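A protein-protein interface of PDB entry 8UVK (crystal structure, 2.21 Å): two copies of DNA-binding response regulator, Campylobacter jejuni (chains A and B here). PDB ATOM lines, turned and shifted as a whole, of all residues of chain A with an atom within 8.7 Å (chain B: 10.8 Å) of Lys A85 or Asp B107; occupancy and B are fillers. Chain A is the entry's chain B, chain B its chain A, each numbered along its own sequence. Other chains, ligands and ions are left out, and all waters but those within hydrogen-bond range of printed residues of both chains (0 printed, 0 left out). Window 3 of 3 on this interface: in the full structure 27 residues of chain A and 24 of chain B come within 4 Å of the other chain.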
ATOM      1  N   LYS A  82     -12.971 -17.660 -11.033  1.00  0.00           N
ATOM      2  CA  LYS A  82     -13.577 -18.301 -12.208  1.00  0.00           C
ATOM      3  C   LYS A  82     -15.017 -17.790 -12.356  1.00  0.00           C
ATOM      4  O   LYS A  82     -15.932 -18.232 -11.650  1.00  0.00           O
ATOM      5  CB  LYS A  82     -13.518 -19.822 -12.104  1.00  0.00           C
ATOM      6  N   ALA A  83     -15.215 -16.843 -13.280  1.00  0.00           N
ATOM      7  CA  ALA A  83     -16.501 -16.204 -13.518  1.00  0.00           C
ATOM      8  C   ALA A  83     -16.970 -16.414 -14.953  1.00  0.00           C
ATOM      9  O   ALA A  83     -17.566 -15.521 -15.561  1.00  0.00           O
ATOM     10  CB  ALA A  83     -16.452 -14.711 -13.194  1.00  0.00           C
ATOM     11  N   ASP A  84     -16.751 -17.611 -15.492  1.00  0.00           N
ATOM     12  CA  ASP A  84     -17.340 -17.950 -16.779  1.00  0.00           C
ATOM     13  C   ASP A  84     -18.860 -18.089 -16.627  1.00  0.00           C
ATOM     14  O   ASP A  84     -19.402 -18.050 -15.518  1.00  0.00           O
ATOM     15  CB  ASP A  84     -16.719 -19.237 -17.344  1.00  0.00           C
ATOM     16  CG  ASP A  84     -16.879 -20.422 -16.411  1.00  0.00           C
ATOM     17  OD1 ASP A  84     -16.054 -20.576 -15.481  1.00  0.00           O
ATOM     18  OD2 ASP A  84     -17.834 -21.197 -16.599  1.00  0.00           O
ATOM     19  N   LYS A  85     -19.567 -18.175 -17.744  1.00  0.00           N
ATOM     20  CA  LYS A  85     -21.028 -18.207 -17.683  1.00  0.00           C
ATOM     21  C   LYS A  85     -21.570 -19.424 -16.959  1.00  0.00           C
ATOM     22  O   LYS A  85     -22.525 -19.323 -16.197  1.00  0.00           O
ATOM     23  CB  LYS A  85     -21.617 -18.138 -19.090  1.00  0.00           C
ATOM     24  CG  LYS A  85     -21.200 -19.272 -20.007  1.00  0.00           C
ATOM     25  CD  LYS A  85     -21.681 -19.013 -21.423  1.00  0.00           C
ATOM     26  CE  LYS A  85     -23.169 -18.712 -21.448  1.00  0.00           C
ATOM     27  NZ  LYS A  85     -23.618 -18.282 -22.799  1.00  0.00           N
ATOM     28  N   ASP A  86     -20.959 -20.573 -17.189  1.00  0.00           N
ATOM     29  CA  ASP A  86     -21.434 -21.790 -16.566  1.00  0.00           C
ATOM     30  C   ASP A  86     -21.394 -21.646 -15.057  1.00  0.00           C
ATOM     31  O   ASP A  86     -22.354 -21.991 -14.371  1.00  0.00           O
ATOM     32  CB  ASP A  86     -20.581 -22.970 -17.014  1.00  0.00           C
ATOM     33  CG  ASP A  86     -20.506 -23.090 -18.522  1.00  0.00           C
ATOM     34  OD1 ASP A  86     -21.341 -22.469 -19.212  1.00  0.00           O
ATOM     35  OD2 ASP A  86     -19.613 -23.807 -19.017  1.00  0.00           O
ATOM     36  N   THR A  87     -20.293 -21.119 -14.538  1.00  0.00           N
ATOM     37  CA  THR A  87     -20.157 -20.955 -13.100  1.00  0.00           C
ATOM     38  C   THR A  87     -21.209 -20.007 -12.549  1.00  0.00           C
ATOM     39  O   THR A  87     -21.881 -20.321 -11.568  1.00  0.00           O
ATOM     40  CB  THR A  87     -18.761 -20.425 -12.733  1.00  0.00           C
ATOM     41  OG1 THR A  87     -17.763 -21.327 -13.226  1.00  0.00           O
ATOM     42  CG2 THR A  87     -18.620 -20.294 -11.225  1.00  0.00           C
ATOM     43  N   GLU A  88     -21.371 -18.854 -13.184  1.00  0.00           N
ATOM     44  CA  GLU A  88     -22.324 -17.873 -12.693  1.00  0.00           C
ATOM     45  C   GLU A  88     -23.720 -18.451 -12.692  1.00  0.00           C
ATOM     46  O   GLU A  88     -24.436 -18.354 -11.701  1.00  0.00           O
ATOM     47  CB  GLU A  88     -22.286 -16.614 -13.556  1.00  0.00           C
ATOM     48  CG  GLU A  88     -23.265 -15.533 -13.127  1.00  0.00           C
ATOM     49  CD  GLU A  88     -23.057 -14.225 -13.868  1.00  0.00           C
ATOM     50  OE1 GLU A  88     -22.153 -14.163 -14.728  1.00  0.00           O
ATOM     51  OE2 GLU A  88     -23.794 -13.257 -13.591  1.00  0.00           O
ATOM     52  N   ILE A  89     -24.102 -19.070 -13.798  1.00  0.00           N
ATOM     53  CA  ILE A  89     -25.442 -19.626 -13.909  1.00  0.00           C
ATOM     54  C   ILE A  89     -25.654 -20.713 -12.870  1.00  0.00           C
ATOM     55  O   ILE A  89     -26.715 -20.797 -12.260  1.00  0.00           O
ATOM     56  CB  ILE A  89     -25.693 -20.181 -15.320  1.00  0.00           C
ATOM     57  CG1 ILE A  89     -25.587 -19.056 -16.351  1.00  0.00           C
ATOM     58  CG2 ILE A  89     -27.055 -20.847 -15.401  1.00  0.00           C
ATOM     59  CD1 ILE A  89     -25.728 -19.520 -17.782  1.00  0.00           C
ATOM     60  N   LYS A  90     -24.636 -21.532 -12.654  1.00  0.00           N
ATOM     61  CA  LYS A  90     -24.744 -22.590 -11.666  1.00  0.00           C
ATOM     62  C   LYS A  90     -25.015 -22.009 -10.292  1.00  0.00           C
ATOM     63  O   LYS A  90     -25.906 -22.470  -9.586  1.00  0.00           O
ATOM     64  CB  LYS A  90     -23.466 -23.418 -11.633  1.00  0.00           C
ATOM     65  CG  LYS A  90     -23.453 -24.471 -10.539  1.00  0.00           C
ATOM     66  CD  LYS A  90     -22.121 -25.200 -10.488  1.00  0.00           C
ATOM     67  CE  LYS A  90     -22.089 -26.200  -9.344  1.00  0.00           C
ATOM     68  NZ  LYS A  90     -20.782 -26.909  -9.263  1.00  0.00           N
ATOM     69  N   ALA A  91     -24.257 -20.989  -9.915  1.00  0.00           N
ATOM     70  CA  ALA A  91     -24.432 -20.383  -8.604  1.00  0.00           C
ATOM     71  C   ALA A  91     -25.820 -19.792  -8.472  1.00  0.00           C
ATOM     72  O   ALA A  91     -26.494 -19.987  -7.462  1.00  0.00           O
ATOM     73  CB  ALA A  91     -23.383 -19.311  -8.377  1.00  0.00           C
ATOM     74  N   LEU A  92     -26.256 -19.078  -9.498  1.00  0.00           N
ATOM     75  CA  LEU A  92     -27.563 -18.452  -9.452  1.00  0.00           C
ATOM     76  C   LEU A  92     -28.640 -19.506  -9.301  1.00  0.00           C
ATOM     77  O   LEU A  92     -29.554 -19.353  -8.494  1.00  0.00           O
ATOM     78  CB  LEU A  92     -27.799 -17.628 -10.714  1.00  0.00           C
ATOM     79  CG  LEU A  92     -26.852 -16.449 -10.934  1.00  0.00           C
ATOM     80  CD1 LEU A  92     -27.142 -15.768 -12.261  1.00  0.00           C
ATOM     81  CD2 LEU A  92     -26.956 -15.460  -9.783  1.00  0.00           C
ATOM     82  N   LYS A  93     -28.529 -20.581 -10.070  1.00  0.00           N
ATOM     83  CA  LYS A  93     -29.520 -21.648 -10.005  1.00  0.00           C
ATOM     84  C   LYS A  93     -29.425 -22.406  -8.693  1.00  0.00           C
ATOM     85  O   LYS A  93     -30.405 -22.989  -8.243  1.00  0.00           O
ATOM     86  CB  LYS A  93     -29.365 -22.594 -11.192  1.00  0.00           C
ATOM     87  CG  LYS A  93     -29.784 -21.972 -12.512  1.00  0.00           C
ATOM     88  CD  LYS A  93     -29.756 -22.987 -13.642  1.00  0.00           C
ATOM     89  CE  LYS A  93     -30.368 -22.411 -14.907  1.00  0.00           C
ATOM     90  NZ  LYS A  93     -31.783 -22.000 -14.695  1.00  0.00           N
ATOM     91  N   PHE A  99     -23.755 -12.875  -8.269  1.00  0.00           N
ATOM     92  CA  PHE A  99     -22.464 -13.494  -8.572  1.00  0.00           C
ATOM     93  C   PHE A  99     -21.558 -12.387  -9.075  1.00  0.00           C
ATOM     94  O   PHE A  99     -21.941 -11.617  -9.962  1.00  0.00           O
ATOM     95  CB  PHE A  99     -22.630 -14.616  -9.610  1.00  0.00           C
ATOM     96  CG  PHE A  99     -21.353 -15.339  -9.959  1.00  0.00           C
ATOM     97  CD1 PHE A  99     -20.913 -16.405  -9.206  1.00  0.00           C
ATOM     98  CD2 PHE A  99     -20.588 -14.935 -11.052  1.00  0.00           C
ATOM     99  CE1 PHE A  99     -19.754 -17.071  -9.530  1.00  0.00           C
ATOM    100  CE2 PHE A  99     -19.411 -15.576 -11.369  1.00  0.00           C
ATOM    101  CZ  PHE A  99     -18.997 -16.654 -10.618  1.00  0.00           C
ATOM    102  N   THR B  16     -35.725 -10.210 -30.343  1.00  0.00           N
ATOM    103  CA  THR B  16     -34.901 -11.242 -29.729  1.00  0.00           C
ATOM    104  C   THR B  16     -35.299 -11.507 -28.280  1.00  0.00           C
ATOM    105  O   THR B  16     -35.724 -12.619 -27.934  1.00  0.00           O
ATOM    106  CB  THR B  16     -33.424 -10.840 -29.860  1.00  0.00           C
ATOM    107  OG1 THR B  16     -33.162 -10.410 -31.213  1.00  0.00           O
ATOM    108  CG2 THR B  16     -32.506 -12.000 -29.501  1.00  0.00           C
ATOM    109  N   ILE B  17     -35.218 -10.462 -27.440  1.00  0.00           N
ATOM    110  CA  ILE B  17     -35.447 -10.600 -25.999  1.00  0.00           C
ATOM    111  C   ILE B  17     -36.796 -11.256 -25.718  1.00  0.00           C
ATOM    112  O   ILE B  17     -36.899 -12.176 -24.895  1.00  0.00           O
ATOM    113  CB  ILE B  17     -35.323  -9.232 -25.311  1.00  0.00           C
ATOM    114  CG1 ILE B  17     -33.904  -8.714 -25.456  1.00  0.00           C
ATOM    115  CG2 ILE B  17     -35.662  -9.351 -23.817  1.00  0.00           C
ATOM    116  CD1 ILE B  17     -33.711  -7.319 -24.992  1.00  0.00           C
ATOM    117  N   ASN B  20     -36.952 -15.031 -26.386  1.00  0.00           N
ATOM    118  CA  ASN B  20     -36.238 -15.802 -25.379  1.00  0.00           C
ATOM    119  C   ASN B  20     -37.088 -15.955 -24.133  1.00  0.00           C
ATOM    120  O   ASN B  20     -37.204 -17.048 -23.583  1.00  0.00           O
ATOM    121  CB  ASN B  20     -34.914 -15.129 -25.035  1.00  0.00           C
ATOM    122  CG  ASN B  20     -33.931 -15.149 -26.187  1.00  0.00           C
ATOM    123  OD1 ASN B  20     -33.331 -16.180 -26.487  1.00  0.00           O
ATOM    124  ND2 ASN B  20     -33.753 -14.004 -26.833  1.00  0.00           N
ATOM    125  N   LEU B  21     -37.690 -14.859 -23.690  1.00  0.00           N
ATOM    126  CA  LEU B  21     -38.511 -14.900 -22.489  1.00  0.00           C
ATOM    127  C   LEU B  21     -39.690 -15.834 -22.669  1.00  0.00           C
ATOM    128  O   LEU B  21     -40.010 -16.621 -21.779  1.00  0.00           O
ATOM    129  CB  LEU B  21     -39.007 -13.499 -22.147  1.00  0.00           C
ATOM    130  CG  LEU B  21     -37.926 -12.474 -21.809  1.00  0.00           C
ATOM    131  CD1 LEU B  21     -38.534 -11.092 -21.633  1.00  0.00           C
ATOM    132  CD2 LEU B  21     -37.168 -12.896 -20.561  1.00  0.00           C
ATOM    133  N   GLU B  23     -39.899 -18.332 -24.679  1.00  0.00           N
ATOM    134  CA  GLU B  23     -39.395 -19.691 -24.704  1.00  0.00           C
ATOM    135  C   GLU B  23     -39.226 -20.195 -23.289  1.00  0.00           C
ATOM    136  O   GLU B  23     -39.585 -21.329 -22.980  1.00  0.00           O
ATOM    137  CB  GLU B  23     -38.060 -19.745 -25.438  1.00  0.00           C
ATOM    138  CG  GLU B  23     -37.327 -21.067 -25.301  1.00  0.00           C
ATOM    139  CD  GLU B  23     -35.944 -21.027 -25.920  1.00  0.00           C
ATOM    140  OE1 GLU B  23     -35.590 -19.991 -26.522  1.00  0.00           O
ATOM    141  OE2 GLU B  23     -35.210 -22.031 -25.804  1.00  0.00           O
ATOM    142  N   PHE B  24     -38.686 -19.351 -22.420  1.00  0.00           N
ATOM    143  CA  PHE B  24     -38.469 -19.747 -21.038  1.00  0.00           C
ATOM    144  C   PHE B  24     -39.788 -20.095 -20.377  1.00  0.00           C
ATOM    145  O   PHE B  24     -39.875 -21.067 -19.630  1.00  0.00           O
ATOM    146  CB  PHE B  24     -37.777 -18.623 -20.269  1.00  0.00           C
ATOM    147  CG  PHE B  24     -37.369 -19.001 -18.874  1.00  0.00           C
ATOM    148  CD1 PHE B  24     -38.301 -19.055 -17.854  1.00  0.00           C
ATOM    149  CD2 PHE B  24     -36.048 -19.294 -18.585  1.00  0.00           C
ATOM    150  CE1 PHE B  24     -37.925 -19.401 -16.570  1.00  0.00           C
ATOM    151  CE2 PHE B  24     -35.665 -19.639 -17.304  1.00  0.00           C
ATOM    152  CZ  PHE B  24     -36.604 -19.693 -16.295  1.00  0.00           C
ATOM    153  N   TYR B  26     -42.339 -17.141 -19.882  1.00  0.00           N
ATOM    154  CA  TYR B  26     -42.742 -15.897 -19.248  1.00  0.00           C
ATOM    155  C   TYR B  26     -43.774 -15.158 -20.062  1.00  0.00           C
ATOM    156  O   TYR B  26     -43.623 -15.021 -21.273  1.00  0.00           O
ATOM    157  CB  TYR B  26     -41.538 -14.969 -19.077  1.00  0.00           C
ATOM    158  CG  TYR B  26     -40.526 -15.392 -18.044  1.00  0.00           C
ATOM    159  CD1 TYR B  26     -40.900 -15.612 -16.727  1.00  0.00           C
ATOM    160  CD2 TYR B  26     -39.187 -15.534 -18.378  1.00  0.00           C
ATOM    161  CE1 TYR B  26     -39.971 -15.987 -15.776  1.00  0.00           C
ATOM    162  CE2 TYR B  26     -38.251 -15.905 -17.433  1.00  0.00           C
ATOM    163  CZ  TYR B  26     -38.649 -16.132 -16.134  1.00  0.00           C
ATOM    164  OH  TYR B  26     -37.722 -16.504 -15.189  1.00  0.00           O
ATOM    165  N   MET B  77     -34.506  -4.174 -14.060  1.00  0.00           N
ATOM    166  CA  MET B  77     -33.199  -4.606 -14.527  1.00  0.00           C
ATOM    167  C   MET B  77     -32.782  -3.717 -15.676  1.00  0.00           C
ATOM    168  O   MET B  77     -33.541  -3.524 -16.621  1.00  0.00           O
ATOM    169  CB  MET B  77     -33.231  -6.065 -14.963  1.00  0.00           C
ATOM    170  CG  MET B  77     -31.911  -6.582 -15.504  1.00  0.00           C
ATOM    171  SD  MET B  77     -31.994  -8.346 -15.856  1.00  0.00           S
ATOM    172  CE  MET B  77     -32.330  -9.001 -14.226  1.00  0.00           C
ATOM    173  N   VAL B 100     -27.464  -5.396 -16.200  1.00  0.00           N
ATOM    174  CA  VAL B 100     -26.952  -6.401 -17.121  1.00  0.00           C
ATOM    175  C   VAL B 100     -26.209  -5.744 -18.264  1.00  0.00           C
ATOM    176  O   VAL B 100     -26.427  -4.571 -18.559  1.00  0.00           O
ATOM    177  CB  VAL B 100     -28.078  -7.282 -17.677  1.00  0.00           C
ATOM    178  CG1 VAL B 100     -28.625  -8.182 -16.582  1.00  0.00           C
ATOM    179  CG2 VAL B 100     -29.180  -6.424 -18.273  1.00  0.00           C
ATOM    180  N   LYS B 101     -25.329  -6.494 -18.913  1.00  0.00           N
ATOM    181  CA  LYS B 101     -24.515  -5.905 -19.968  1.00  0.00           C
ATOM    182  C   LYS B 101     -24.824  -6.423 -21.357  1.00  0.00           C
ATOM    183  O   LYS B 101     -24.900  -7.630 -21.571  1.00  0.00           O
ATOM    184  CB  LYS B 101     -23.032  -6.138 -19.671  1.00  0.00           C
ATOM    185  N   PRO B 103     -23.622  -6.417 -25.526  1.00  0.00           N
ATOM    186  CA  PRO B 103     -24.333  -7.580 -26.100  1.00  0.00           C
ATOM    187  C   PRO B 103     -24.752  -8.598 -25.050  1.00  0.00           C
ATOM    188  O   PRO B 103     -24.021  -8.967 -24.131  1.00  0.00           O
ATOM    189  CB  PRO B 103     -23.310  -8.154 -27.104  1.00  0.00           C
ATOM    190  CG  PRO B 103     -21.974  -7.647 -26.612  1.00  0.00           C
ATOM    191  CD  PRO B 103     -22.290  -6.266 -26.148  1.00  0.00           C
ATOM    192  N   LEU B 104     -26.009  -8.999 -25.132  1.00  0.00           N
ATOM    193  CA  LEU B 104     -26.619  -9.724 -24.034  1.00  0.00           C
ATOM    194  C   LEU B 104     -26.261 -11.193 -24.126  1.00  0.00           C
ATOM    195  O   LEU B 104     -26.363 -11.802 -25.199  1.00  0.00           O
ATOM    196  CB  LEU B 104     -28.137  -9.536 -24.043  1.00  0.00           C
ATOM    197  CG  LEU B 104     -28.670  -8.140 -23.710  1.00  0.00           C
ATOM    198  CD1 LEU B 104     -30.194  -8.091 -23.866  1.00  0.00           C
ATOM    199  CD2 LEU B 104     -28.276  -7.771 -22.279  1.00  0.00           C
ATOM    200  N   ASP B 105     -25.825 -11.755 -23.004  1.00  0.00           N
ATOM    201  CA  ASP B 105     -25.744 -13.199 -22.847  1.00  0.00           C
ATOM    202  C   ASP B 105     -27.096 -13.693 -22.353  1.00  0.00           C
ATOM    203  O   ASP B 105     -27.443 -13.486 -21.184  1.00  0.00           O
ATOM    204  CB  ASP B 105     -24.636 -13.576 -21.871  1.00  0.00           C
ATOM    205  CG  ASP B 105     -24.397 -15.053 -21.837  1.00  0.00           C
ATOM    206  OD1 ASP B 105     -25.348 -15.834 -22.097  1.00  0.00           O
ATOM    207  OD2 ASP B 105     -23.227 -15.435 -21.605  1.00  0.00           O
ATOM    208  N   PHE B 106     -27.854 -14.378 -23.212  1.00  0.00           N
ATOM    209  CA  PHE B 106     -29.199 -14.717 -22.774  1.00  0.00           C
ATOM    210  C   PHE B 106     -29.243 -15.903 -21.815  1.00  0.00           C
ATOM    211  O   PHE B 106     -30.219 -16.033 -21.063  1.00  0.00           O
ATOM    212  CB  PHE B 106     -30.110 -14.975 -23.952  1.00  0.00           C
ATOM    213  CG  PHE B 106     -30.225 -13.812 -24.871  1.00  0.00           C
ATOM    214  CD1 PHE B 106     -29.320 -13.633 -25.906  1.00  0.00           C
ATOM    215  CD2 PHE B 106     -31.321 -12.970 -24.786  1.00  0.00           C
ATOM    216  CE1 PHE B 106     -29.467 -12.581 -26.790  1.00  0.00           C
ATOM    217  CE2 PHE B 106     -31.459 -11.908 -25.640  1.00  0.00           C
ATOM    218  CZ  PHE B 106     -30.544 -11.715 -26.651  1.00  0.00           C
ATOM    219  N   ASP B 107     -28.203 -16.742 -21.798  1.00  0.00           N
ATOM    220  CA  ASP B 107     -28.099 -17.782 -20.777  1.00  0.00           C
ATOM    221  C   ASP B 107     -27.906 -17.172 -19.389  1.00  0.00           C
ATOM    222  O   ASP B 107     -28.499 -17.627 -18.404  1.00  0.00           O
ATOM    223  CB  ASP B 107     -26.942 -18.713 -21.115  1.00  0.00           C
ATOM    224  CG  ASP B 107     -27.030 -19.265 -22.518  1.00  0.00           C
ATOM    225  OD1 ASP B 107     -28.055 -19.902 -22.882  1.00  0.00           O
ATOM    226  OD2 ASP B 107     -26.064 -19.035 -23.278  1.00  0.00           O
ATOM    227  N   ILE B 108     -27.088 -16.138 -19.295  1.00  0.00           N
ATOM    228  CA  ILE B 108     -26.889 -15.493 -18.010  1.00  0.00           C
ATOM    229  C   ILE B 108     -28.112 -14.669 -17.639  1.00  0.00           C
ATOM    230  O   ILE B 108     -28.558 -14.694 -16.494  1.00  0.00           O
ATOM    231  CB  ILE B 108     -25.639 -14.599 -18.013  1.00  0.00           C
ATOM    232  CG1 ILE B 108     -24.396 -15.432 -18.323  1.00  0.00           C
ATOM    233  CG2 ILE B 108     -25.486 -13.892 -16.676  1.00  0.00           C
ATOM    234  CD1 ILE B 108     -23.104 -14.649 -18.243  1.00  0.00           C
ATOM    235  N   LEU B 109     -28.665 -13.952 -18.608  1.00  0.00           N
ATOM    236  CA  LEU B 109     -29.811 -13.101 -18.331  1.00  0.00           C
ATOM    237  C   LEU B 109     -30.952 -13.908 -17.760  1.00  0.00           C
ATOM    238  O   LEU B 109     -31.513 -13.555 -16.726  1.00  0.00           O
ATOM    239  CB  LEU B 109     -30.270 -12.410 -19.609  1.00  0.00           C
ATOM    240  CG  LEU B 109     -31.493 -11.502 -19.503  1.00  0.00           C
ATOM    241  CD1 LEU B 109     -31.226 -10.371 -18.524  1.00  0.00           C
ATOM    242  CD2 LEU B 109     -31.860 -10.950 -20.872  1.00  0.00           C
ATOM    243  N   LEU B 110     -31.293 -15.005 -18.422  1.00  0.00           N
ATOM    244  CA  LEU B 110     -32.399 -15.823 -17.965  1.00  0.00           C
ATOM    245  C   LEU B 110     -32.141 -16.320 -16.557  1.00  0.00           C
ATOM    246  O   LEU B 110     -33.058 -16.401 -15.744  1.00  0.00           O
ATOM    247  CB  LEU B 110     -32.627 -16.998 -18.913  1.00  0.00           C
ATOM    248  CG  LEU B 110     -33.283 -16.645 -20.247  1.00  0.00           C
ATOM    249  CD1 LEU B 110     -33.429 -17.883 -21.116  1.00  0.00           C
ATOM    250  CD2 LEU B 110     -34.636 -15.988 -20.015  1.00  0.00           C
ATOM    251  N   ALA B 111     -30.890 -16.649 -16.266  1.00  0.00           N
ATOM    252  CA  ALA B 111     -30.549 -17.106 -14.922  1.00  0.00           C
ATOM    253  C   ALA B 111     -30.714 -15.999 -13.877  1.00  0.00           C
ATOM    254  O   ALA B 111     -31.161 -16.276 -12.760  1.00  0.00           O
ATOM    255  CB  ALA B 111     -29.124 -17.647 -14.880  1.00  0.00           C
ATOM    256  N   ARG B 112     -30.379 -14.765 -14.230  1.00  0.00           N
ATOM    257  CA  ARG B 112     -30.514 -13.664 -13.290  1.00  0.00           C
ATOM    258  C   ARG B 112     -31.975 -13.318 -13.061  1.00  0.00           C
ATOM    259  O   ARG B 112     -32.393 -13.092 -11.930  1.00  0.00           O
ATOM    260  CB  ARG B 112     -29.741 -12.436 -13.774  1.00  0.00           C
ATOM    261  CG  ARG B 112     -28.237 -12.572 -13.624  1.00  0.00           C
ATOM    262  CD  ARG B 112     -27.529 -11.239 -13.784  1.00  0.00           C
ATOM    263  NE  ARG B 112     -26.154 -11.310 -13.301  1.00  0.00           N
ATOM    264  CZ  ARG B 112     -25.794 -11.068 -12.044  1.00  0.00           C
ATOM    265  NH1 ARG B 112     -26.708 -10.734 -11.144  1.00  0.00           N
ATOM    266  NH2 ARG B 112     -24.522 -11.160 -11.687  1.00  0.00           N
ATOM    267  N   ILE B 113     -32.756 -13.284 -14.133  1.00  0.00           N
ATOM    268  CA  ILE B 113     -34.172 -12.996 -14.000  1.00  0.00           C
ATOM    269  C   ILE B 113     -34.795 -14.037 -13.101  1.00  0.00           C
ATOM    270  O   ILE B 113     -35.556 -13.712 -12.194  1.00  0.00           O
ATOM    271  CB  ILE B 113     -34.873 -13.000 -15.363  1.00  0.00           C
ATOM    272  CG1 ILE B 113     -34.312 -11.881 -16.240  1.00  0.00           C
ATOM    273  CG2 ILE B 113     -36.375 -12.845 -15.191  1.00  0.00           C
ATOM    274  CD1 ILE B 113     -34.935 -11.809 -17.615  1.00  0.00           C
ATOM    275  N   GLU B 114     -34.457 -15.295 -13.339  1.00  0.00           N
ATOM    276  CA  GLU B 114     -34.964 -16.359 -12.497  1.00  0.00           C
ATOM    277  C   GLU B 114     -34.637 -16.063 -11.045  1.00  0.00           C
ATOM    278  O   GLU B 114     -35.530 -15.998 -10.203  1.00  0.00           O
ATOM    279  CB  GLU B 114     -34.355 -17.692 -12.913  1.00  0.00           C
ATOM    280  CG  GLU B 114     -34.861 -18.885 -12.124  1.00  0.00           C
ATOM    281  CD  GLU B 114     -34.146 -20.163 -12.505  1.00  0.00           C
ATOM    282  OE1 GLU B 114     -33.138 -20.080 -13.234  1.00  0.00           O
ATOM    283  OE2 GLU B 114     -34.592 -21.249 -12.079  1.00  0.00           O
ATOM    284  N   ALA B 115     -33.356 -15.878 -10.750  1.00  0.00           N
ATOM    285  CA  ALA B 115     -32.954 -15.590  -9.378  1.00  0.00           C
ATOM    286  C   ALA B 115     -33.660 -14.352  -8.840  1.00  0.00           C
ATOM    287  O   ALA B 115     -33.993 -14.288  -7.651  1.00  0.00           O
ATOM    288  CB  ALA B 115     -31.428 -15.423  -9.303  1.00  0.00           C
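NZ of Lys A93 is in salt-bridge range of OE1 of Glu B114, at 2.8 Å.
O of Phe A99 is in hydrogen-bond range of NH2 of Arg B112 (3.1 Å).
The guanidinium group of Arg B112 is in salt-bridge range of the side-chain carboxylate of Glu A88 (2.9 Å).
The side-chain carboxylate (OD2) of Asp B107 lies within salt-bridge range of the side-chain amino group (NZ) of Lys A85 (2.6 Å).
The side-chain carboxylate of Asp B105 lies within salt-bridge range of the side-chain amino group of Lys A85 (3.1 Å).
The backbone NH (N) of Asp B107 sits at hydrogen-bond distance from the side-chain carboxylate (OD1) of Asp B105 (3.0 Å).
The backbone NH (N) of Ile B108 is in hydrogen-bond range of the side-chain carboxylate (OD1) of Asp B105 (3.3 Å).
Ile B108 touches Lys A85.
Glu A88 touches Ile B108 (OE2 to CG2, 3.6 Å).
O of Asp B107 touches CD1 of Ile A89 (3.4 Å).
CD1 of Ile A89 touches N of Ile B108 (3.9 Å).
Ile A89 touches Ala B111 (CG2 to CB, 3.8 Å).
Leu A92 touches Ala B111.
Arg B112 touches Leu A92 (CG to CD1, 3.6 Å).
No residue of chain B comes within 4 Å of Asp A84.
Lys A85 touches three residues of chain B.
No residue of chain B comes within 4 Å of Asp A86.
No residue of chain B comes within 4 Å of Thr A87.
Printed residues of chain B within 4 Å of Glu A88: Ile B108 (3.6 Å) and Arg B112 (2.9 Å).
Ile A89 touches just these residues of chain B: Asp B107 (3.4 Å), Ile B108 (3.9 Å) and Ala B111 (3.8 Å).
Of chain A, only Lys A85 and Ile A89 come within 4 Å of Asp B107.
Of the printed residues of chain A, Ile B108 touches Lys A85 (3.9 Å), Glu A88 (3.6 Å) and Ile A89 (3.9 Å).
Printed residues of chain A within 4 Å of Arg B112: Glu A88 (2.9 Å), Leu A92 (3.6 Å) and Phe A99 (3.1 Å).
Of the printed residues of chain A, Glu B114 touches Lys A93.
The nearest residue of chain B that does not touch Lys A85 is Phe B106 (5.8 Å).
The nearest printed residue of chain A that does not touch Ala B111 is Lys A93 (4.9 Å).
Of the 13 printed residues of chain A, 6 touch a printed residue of chain B.
Hydrophobic or aromatic side chains of chain A that line the printed part of chain B: Ile A89 and Leu A92.
Hydrophobic or aromatic side chains of chain B that line the printed part of chain A: Ile B108 and Ala B111.
Among the printed residues, 12 pairs touch across the chains.
Among the printed residues, Asp or Glu carboxylates within 4 Å of a Lys or Arg side-chain nitrogen of the other chain: Lys A85 with Asp B105, Lys A85 with Asp B107, Glu A88 with Arg B112 and Lys A93 with Glu B114.
No position is printed for both chains.
Of the 12 pairs that touch across the chains among the printed residues, none has its exchanged pair printed and touching as well.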
